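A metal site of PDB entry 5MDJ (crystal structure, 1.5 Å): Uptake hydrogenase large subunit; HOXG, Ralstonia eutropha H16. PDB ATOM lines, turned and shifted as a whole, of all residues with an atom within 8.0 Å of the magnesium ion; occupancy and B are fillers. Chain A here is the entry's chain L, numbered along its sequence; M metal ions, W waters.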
ATOM      1  N   TRP A  52     -19.519  29.353  14.216  1.00  0.00           N
ATOM      2  CA  TRP A  52     -20.477  28.377  13.745  1.00  0.00           C
ATOM      3  C   TRP A  52     -21.444  28.080  14.894  1.00  0.00           C
ATOM      4  O   TRP A  52     -21.033  28.070  16.049  1.00  0.00           O
ATOM      5  CB  TRP A  52     -19.763  27.082  13.308  1.00  0.00           C
ATOM      6  CG  TRP A  52     -20.689  26.001  12.878  1.00  0.00           C
ATOM      7  CD1 TRP A  52     -21.526  26.016  11.799  1.00  0.00           C
ATOM      8  CD2 TRP A  52     -20.880  24.739  13.516  1.00  0.00           C
ATOM      9  NE1 TRP A  52     -22.246  24.853  11.727  1.00  0.00           N
ATOM     10  CE2 TRP A  52     -21.852  24.035  12.766  1.00  0.00           C
ATOM     11  CE3 TRP A  52     -20.312  24.117  14.636  1.00  0.00           C
ATOM     12  CZ2 TRP A  52     -22.290  22.773  13.110  1.00  0.00           C
ATOM     13  CZ3 TRP A  52     -20.760  22.858  14.981  1.00  0.00           C
ATOM     14  CH2 TRP A  52     -21.730  22.194  14.219  1.00  0.00           C
ATOM     15  N   GLU A  56     -28.546  24.035  11.018  1.00  0.00           N
ATOM     16  CA  GLU A  56     -29.075  22.995  10.132  1.00  0.00           C
ATOM     17  C   GLU A  56     -29.434  21.718  10.918  1.00  0.00           C
ATOM     18  O   GLU A  56     -30.502  21.166  10.714  1.00  0.00           O
ATOM     19  CB  GLU A  56     -28.101  22.697   8.987  1.00  0.00           C
ATOM     20  CG  GLU A  56     -27.970  23.850   7.986  1.00  0.00           C
ATOM     21  CD  GLU A  56     -26.659  23.870   7.219  1.00  0.00           C
ATOM     22  OE1 GLU A  56     -25.616  23.440   7.753  1.00  0.00           O
ATOM     23  OE2 GLU A  56     -26.660  24.391   6.059  1.00  0.00           O
ATOM     24  N   ILE A  74     -30.722  32.869  11.856  1.00  0.00           N
ATOM     25  CA  ILE A  74     -29.400  32.836  11.250  1.00  0.00           C
ATOM     26  C   ILE A  74     -28.802  34.240  11.303  1.00  0.00           C
ATOM     27  O   ILE A  74     -27.604  34.384  11.467  1.00  0.00           O
ATOM     28  CB  ILE A  74     -29.439  32.300   9.804  1.00  0.00           C
ATOM     29  CG1 ILE A  74     -29.708  30.800   9.847  1.00  0.00           C
ATOM     30  CG2 ILE A  74     -28.138  32.615   9.081  1.00  0.00           C
ATOM     31  CD1 ILE A  74     -30.008  30.144   8.522  1.00  0.00           C
ATOM     32  N   GLU A 347     -21.694  21.883  -2.537  1.00  0.00           N
ATOM     33  CA  GLU A 347     -20.800  22.389  -1.510  1.00  0.00           C
ATOM     34  C   GLU A 347     -19.705  21.404  -1.167  1.00  0.00           C
ATOM     35  O   GLU A 347     -19.987  20.234  -0.846  1.00  0.00           O
ATOM     36  CB  GLU A 347     -21.542  22.728  -0.235  1.00  0.00           C
ATOM     37  CG  GLU A 347     -22.476  23.931  -0.397  1.00  0.00           C
ATOM     38  CD  GLU A 347     -23.171  24.247   0.900  1.00  0.00           C
ATOM     39  OE1 GLU A 347     -23.966  23.393   1.357  1.00  0.00           O
ATOM     40  OE2 GLU A 347     -22.908  25.340   1.454  1.00  0.00           O
ATOM     41  N   TYR A 354     -15.405  20.754   8.571  1.00  0.00           N
ATOM     42  CA  TYR A 354     -16.463  19.738   8.545  1.00  0.00           C
ATOM     43  C   TYR A 354     -15.885  18.469   7.967  1.00  0.00           C
ATOM     44  O   TYR A 354     -14.750  18.460   7.505  1.00  0.00           O
ATOM     45  CB  TYR A 354     -17.642  20.165   7.681  1.00  0.00           C
ATOM     46  CG  TYR A 354     -18.214  21.487   8.068  1.00  0.00           C
ATOM     47  CD1 TYR A 354     -19.082  21.591   9.150  1.00  0.00           C
ATOM     48  CD2 TYR A 354     -17.859  22.649   7.401  1.00  0.00           C
ATOM     49  CE1 TYR A 354     -19.602  22.816   9.541  1.00  0.00           C
ATOM     50  CE2 TYR A 354     -18.382  23.869   7.784  1.00  0.00           C
ATOM     51  CZ  TYR A 354     -19.258  23.957   8.841  1.00  0.00           C
ATOM     52  OH  TYR A 354     -19.782  25.167   9.244  1.00  0.00           O
ATOM     53  N   PRO A 365     -27.453  20.437  -1.979  1.00  0.00           N
ATOM     54  CA  PRO A 365     -27.901  20.607  -0.603  1.00  0.00           C
ATOM     55  C   PRO A 365     -29.006  19.649  -0.127  1.00  0.00           C
ATOM     56  O   PRO A 365     -29.157  19.442   1.087  1.00  0.00           O
ATOM     57  CB  PRO A 365     -28.350  22.065  -0.568  1.00  0.00           C
ATOM     58  CG  PRO A 365     -27.471  22.734  -1.571  1.00  0.00           C
ATOM     59  CD  PRO A 365     -27.452  21.733  -2.696  1.00  0.00           C
ATOM     60  N   GLY A 368     -27.015  17.323   1.538  1.00  0.00           N
ATOM     61  CA  GLY A 368     -25.979  17.993   2.299  1.00  0.00           C
ATOM     62  C   GLY A 368     -25.779  17.411   3.697  1.00  0.00           C
ATOM     63  O   GLY A 368     -26.701  16.824   4.278  1.00  0.00           O
ATOM     64  N   VAL A 369     -24.574  17.608   4.214  1.00  0.00           N
ATOM     65  CA  VAL A 369     -24.132  17.058   5.501  1.00  0.00           C
ATOM     66  C   VAL A 369     -23.374  18.124   6.261  1.00  0.00           C
ATOM     67  O   VAL A 369     -22.467  18.778   5.718  1.00  0.00           O
ATOM     68  CB  VAL A 369     -23.206  15.837   5.290  1.00  0.00           C
ATOM     69  CG1 VAL A 369     -22.670  15.325   6.632  1.00  0.00           C
ATOM     70  CG2 VAL A 369     -23.935  14.729   4.533  1.00  0.00           C
ATOM     71  N   THR A 370     -23.720  18.317   7.530  1.00  0.00           N
ATOM     72  CA  THR A 370     -23.018  19.253   8.387  1.00  0.00           C
ATOM     73  C   THR A 370     -22.556  18.570   9.687  1.00  0.00           C
ATOM     74  O   THR A 370     -23.267  18.539  10.688  1.00  0.00           O
ATOM     75  CB  THR A 370     -23.911  20.475   8.684  1.00  0.00           C
ATOM     76  OG1 THR A 370     -24.406  21.011   7.447  1.00  0.00           O
ATOM     77  CG2 THR A 370     -23.131  21.554   9.417  1.00  0.00           C
ATOM     78  N   TRP A 398     -14.977  27.938   9.075  1.00  0.00           N
ATOM     79  CA  TRP A 398     -16.316  27.402   9.314  1.00  0.00           C
ATOM     80  C   TRP A 398     -17.272  27.548   8.109  1.00  0.00           C
ATOM     81  O   TRP A 398     -18.402  27.067   8.149  1.00  0.00           O
ATOM     82  CB  TRP A 398     -16.934  28.008  10.593  1.00  0.00           C
ATOM     83  CG  TRP A 398     -16.327  27.478  11.863  1.00  0.00           C
ATOM     84  CD1 TRP A 398     -15.538  28.161  12.746  1.00  0.00           C
ATOM     85  CD2 TRP A 398     -16.452  26.140  12.379  1.00  0.00           C
ATOM     86  NE1 TRP A 398     -15.174  27.344  13.795  1.00  0.00           N
ATOM     87  CE2 TRP A 398     -15.706  26.096  13.579  1.00  0.00           C
ATOM     88  CE3 TRP A 398     -17.116  24.986  11.944  1.00  0.00           C
ATOM     89  CZ2 TRP A 398     -15.629  24.941  14.368  1.00  0.00           C
ATOM     90  CZ3 TRP A 398     -17.029  23.828  12.732  1.00  0.00           C
ATOM     91  CH2 TRP A 398     -16.275  23.816  13.909  1.00  0.00           C
ATOM     92  N   ILE A 399     -16.823  28.200   7.027  1.00  0.00           N
ATOM     93  CA  ILE A 399     -17.652  28.391   5.863  1.00  0.00           C
ATOM     94  C   ILE A 399     -17.406  27.218   4.900  1.00  0.00           C
ATOM     95  O   ILE A 399     -16.242  26.888   4.633  1.00  0.00           O
ATOM     96  CB  ILE A 399     -17.320  29.742   5.174  1.00  0.00           C
ATOM     97  CG1 ILE A 399     -17.409  30.896   6.170  1.00  0.00           C
ATOM     98  CG2 ILE A 399     -18.248  29.958   3.992  1.00  0.00           C
ATOM     99  CD1 ILE A 399     -16.900  32.213   5.626  1.00  0.00           C
ATOM    100  N   LYS A 400     -18.490  26.594   4.405  1.00  0.00           N
ATOM    101  CA  LYS A 400     -18.388  25.597   3.335  1.00  0.00           C
ATOM    102  C   LYS A 400     -18.023  26.281   1.994  1.00  0.00           C
ATOM    103  O   LYS A 400     -18.011  27.518   1.902  1.00  0.00           O
ATOM    104  CB  LYS A 400     -19.694  24.801   3.173  1.00  0.00           C
ATOM    105  CG  LYS A 400     -20.093  23.973   4.382  1.00  0.00           C
ATOM    106  CD  LYS A 400     -21.249  23.031   4.029  1.00  0.00           C
ATOM    107  CE  LYS A 400     -21.724  22.174   5.219  1.00  0.00           C
ATOM    108  NZ  LYS A 400     -23.055  21.603   4.906  1.00  0.00           N
ATOM    109  N   PRO A 402     -19.336  26.540  -1.644  1.00  0.00           N
ATOM    110  CA  PRO A 402     -20.303  26.303  -2.724  1.00  0.00           C
ATOM    111  C   PRO A 402     -19.692  26.602  -4.096  1.00  0.00           C
ATOM    112  O   PRO A 402     -18.901  27.555  -4.248  1.00  0.00           O
ATOM    113  CB  PRO A 402     -21.431  27.316  -2.442  1.00  0.00           C
ATOM    114  CG  PRO A 402     -21.150  27.867  -1.060  1.00  0.00           C
ATOM    115  CD  PRO A 402     -19.647  27.796  -0.927  1.00  0.00           C
ATOM    116  N   GLY A 534     -30.355  30.081  -0.821  1.00  0.00           N
ATOM    117  CA  GLY A 534     -31.271  28.959  -0.963  1.00  0.00           C
ATOM    118  C   GLY A 534     -31.386  28.156   0.319  1.00  0.00           C
ATOM    119  O   GLY A 534     -30.402  28.006   1.057  1.00  0.00           O
ATOM    120  N   TRP A 536     -32.878  24.267   1.239  1.00  0.00           N
ATOM    121  CA  TRP A 536     -33.307  22.973   0.689  1.00  0.00           C
ATOM    122  C   TRP A 536     -33.801  22.128   1.854  1.00  0.00           C
ATOM    123  O   TRP A 536     -33.056  21.890   2.807  1.00  0.00           O
ATOM    124  CB  TRP A 536     -32.161  22.249  -0.014  1.00  0.00           C
ATOM    125  CG  TRP A 536     -31.751  22.818  -1.361  1.00  0.00           C
ATOM    126  CD1 TRP A 536     -32.088  22.304  -2.601  1.00  0.00           C
ATOM    127  CD2 TRP A 536     -30.954  23.985  -1.631  1.00  0.00           C
ATOM    128  NE1 TRP A 536     -31.513  23.045  -3.597  1.00  0.00           N
ATOM    129  CE2 TRP A 536     -30.830  24.086  -3.028  1.00  0.00           C
ATOM    130  CE3 TRP A 536     -30.305  24.936  -0.827  1.00  0.00           C
ATOM    131  CZ2 TRP A 536     -30.087  25.096  -3.659  1.00  0.00           C
ATOM    132  CZ3 TRP A 536     -29.573  25.938  -1.437  1.00  0.00           C
ATOM    133  CH2 TRP A 536     -29.471  26.011  -2.847  1.00  0.00           C
ATOM    134  N   TYR A 547     -32.338  19.717   6.394  1.00  0.00           N
ATOM    135  CA  TYR A 547     -32.486  21.135   6.125  1.00  0.00           C
ATOM    136  C   TYR A 547     -31.101  21.710   5.885  1.00  0.00           C
ATOM    137  O   TYR A 547     -30.258  21.658   6.767  1.00  0.00           O
ATOM    138  CB  TYR A 547     -33.190  21.836   7.291  1.00  0.00           C
ATOM    139  CG  TYR A 547     -33.839  23.146   6.887  1.00  0.00           C
ATOM    140  CD1 TYR A 547     -33.089  24.247   6.502  1.00  0.00           C
ATOM    141  CD2 TYR A 547     -35.231  23.275   6.901  1.00  0.00           C
ATOM    142  CE1 TYR A 547     -33.713  25.437   6.114  1.00  0.00           C
ATOM    143  CE2 TYR A 547     -35.852  24.438   6.528  1.00  0.00           C
ATOM    144  CZ  TYR A 547     -35.092  25.532   6.156  1.00  0.00           C
ATOM    145  OH  TYR A 547     -35.744  26.700   5.778  1.00  0.00           O
ATOM    146  N   GLN A 548     -30.852  22.202   4.673  1.00  0.00           N
ATOM    147  CA  GLN A 548     -29.546  22.730   4.353  1.00  0.00           C
ATOM    148  C   GLN A 548     -29.682  24.099   3.710  1.00  0.00           C
ATOM    149  O   GLN A 548     -30.516  24.304   2.818  1.00  0.00           O
ATOM    150  CB  GLN A 548     -28.810  21.804   3.397  1.00  0.00           C
ATOM    151  CG  GLN A 548     -28.360  20.508   4.051  1.00  0.00           C
ATOM    152  CD  GLN A 548     -27.082  20.634   4.854  1.00  0.00           C
ATOM    153  OE1 GLN A 548     -26.130  21.284   4.431  1.00  0.00           O
ATOM    154  NE2 GLN A 548     -27.053  19.981   6.011  1.00  0.00           N
ATOM    155  N   CYS A 549     -28.851  25.016   4.172  1.00  0.00           N
ATOM    156  CA  CYS A 549     -28.826  26.392   3.690  1.00  0.00           C
ATOM    157  C   CYS A 549     -27.503  26.669   2.994  1.00  0.00           C
ATOM    158  O   CYS A 549     -26.423  26.290   3.510  1.00  0.00           O
ATOM    159  CB  CYS A 549     -28.948  27.361   4.856  1.00  0.00           C
ATOM    160  SG  CYS A 549     -30.403  27.103   5.910  1.00  0.00           S
ATOM    161  N   VAL A 550     -27.584  27.355   1.846  1.00  0.00           N
ATOM    162  CA  VAL A 550     -26.423  27.864   1.173  1.00  0.00           C
ATOM    163  C   VAL A 550     -26.713  29.365   0.986  1.00  0.00           C
ATOM    164  O   VAL A 550     -27.669  29.735   0.289  1.00  0.00           O
ATOM    165  CB  VAL A 550     -26.165  27.200  -0.184  1.00  0.00           C
ATOM    166  CG1 VAL A 550     -24.810  27.614  -0.741  1.00  0.00           C
ATOM    167  CG2 VAL A 550     -26.225  25.686  -0.043  1.00  0.00           C
ATOM    168  N   VAL A 551     -25.881  30.170   1.612  1.00  0.00           N
ATOM    169  CA  VAL A 551     -26.182  31.563   1.916  1.00  0.00           C
ATOM    170  C   VAL A 551     -25.206  32.447   1.103  1.00  0.00           C
ATOM    171  O   VAL A 551     -24.113  31.983   0.722  1.00  0.00           O
ATOM    172  CB  VAL A 551     -26.119  31.741   3.448  1.00  0.00           C
ATOM    173  CG1 VAL A 551     -26.529  33.099   3.930  1.00  0.00           C
ATOM    174  CG2 VAL A 551     -27.016  30.702   4.122  1.00  0.00           C
ATOM    175  N   THR A 554     -21.743  32.581   2.253  1.00  0.00           N
ATOM    176  CA  THR A 554     -21.121  31.247   2.050  1.00  0.00           C
ATOM    177  C   THR A 554     -20.432  31.185   0.688  1.00  0.00           C
ATOM    178  O   THR A 554     -19.278  30.739   0.590  1.00  0.00           O
ATOM    179  CB  THR A 554     -22.138  30.088   2.158  1.00  0.00           C
ATOM    180  OG1 THR A 554     -23.039  30.308   3.252  1.00  0.00           O
ATOM    181  CG2 THR A 554     -21.405  28.766   2.323  1.00  0.00           C
ATOM    182  N   CYS A 600     -24.554  34.653   8.747  1.00  0.00           N
ATOM    183  CA  CYS A 600     -25.185  34.064   7.574  1.00  0.00           C
ATOM    184  C   CYS A 600     -24.315  32.984   6.932  1.00  0.00           C
ATOM    185  O   CYS A 600     -24.789  31.935   6.542  1.00  0.00           O
ATOM    186  CB  CYS A 600     -25.437  35.121   6.502  1.00  0.00           C
ATOM    187  SG  CYS A 600     -27.095  35.815   6.567  1.00  0.00           S
ATOM    188  N   SER A 601     -23.038  33.311   6.779  1.00  0.00           N
ATOM    189  CA  SER A 601     -22.150  32.421   6.006  1.00  0.00           C
ATOM    190  C   SER A 601     -22.027  31.009   6.582  1.00  0.00           C
ATOM    191  O   SER A 601     -21.848  30.066   5.818  1.00  0.00           O
ATOM    192  CB  SER A 601     -20.752  33.017   5.821  1.00  0.00           C
ATOM    193  OG  SER A 601     -19.986  32.948   6.993  1.00  0.00           O
ATOM    194  N   THR A 602     -22.119  30.903   7.911  1.00  0.00           N
ATOM    195  CA  THR A 602     -21.863  29.645   8.618  1.00  0.00           C
ATOM    196  C   THR A 602     -23.109  29.003   9.229  1.00  0.00           C
ATOM    197  O   THR A 602     -23.187  27.777   9.275  1.00  0.00           O
ATOM    198  CB  THR A 602     -20.840  29.907   9.738  1.00  0.00           C
ATOM    199  OG1 THR A 602     -21.332  30.918  10.624  1.00  0.00           O
ATOM    200  CG2 THR A 602     -19.503  30.341   9.149  1.00  0.00           C
ATOM    201  N   HIS A 603     -24.065  29.810   9.675  1.00  0.00           N
ATOM    202  CA  HIS A 603     -25.348  29.336  10.209  1.00  0.00           C
ATOM    203  C   HIS A 603     -25.163  28.133  11.149  1.00  0.00           C
ATOM    204  O   HIS A 603     -25.848  27.108  11.055  1.00  0.00           O
ATOM    205  CB  HIS A 603     -26.394  29.097   9.095  1.00  0.00           C
ATOM    206  CG  HIS A 603     -25.860  28.452   7.854  1.00  0.00           C
ATOM    207  ND1 HIS A 603     -25.212  29.159   6.855  1.00  0.00           N
ATOM    208  CD2 HIS A 603     -25.936  27.181   7.419  1.00  0.00           C
ATOM    209  CE1 HIS A 603     -24.860  28.322   5.898  1.00  0.00           C
ATOM    210  NE2 HIS A 603     -25.293  27.120   6.204  1.00  0.00           N
ATOM    211  OXT HIS A 603     -24.262  28.228  11.996  1.00  0.00           O
HETATM  212 MG    MG M   1     -25.112  25.302   4.873  1.00  0.00          MG
HETATM  213  O   HOH W   1     -23.724  24.406   6.253  1.00  0.00           O
HETATM  214  O   HOH W   2     -25.061  23.622   3.746  1.00  0.00           O
HETATM  215  O   HOH W   3     -23.525  26.198   3.878  1.00  0.00           O
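The magnesium ion is bound by water W2 (2.0 Å), water W3 (2.1 Å), O of Cys 549 (2.1 Å), OE2 of Glu 56 (2.2 Å), water W1 (2.2 Å) and NE2 of His 603 (2.3 Å).
The magnesium ion has six donor atoms within binding distance.
The nearest printed residue that does not touch the magnesium ion is Glu 347 (4.1 Å).
OE1 of Glu 56 lies within hydrogen-bond range of OG1 of Thr 370, 2.7 Å away.
The backbone carbonyl oxygen of Cys 600 is in hydrogen-bond range of a ring nitrogen (ND1) of His 603.
Water W1 bridges the side-chain carboxylate (OE1) of Glu 56 and the side-chain amino group (NZ) of Lys 400.
Water W2 lies within hydrogen-bond range of OE1 of Glu 347 (2.6 Å), OE1 of Gln 548 (2.7 Å) and NZ of Lys 400 (3.1 Å).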
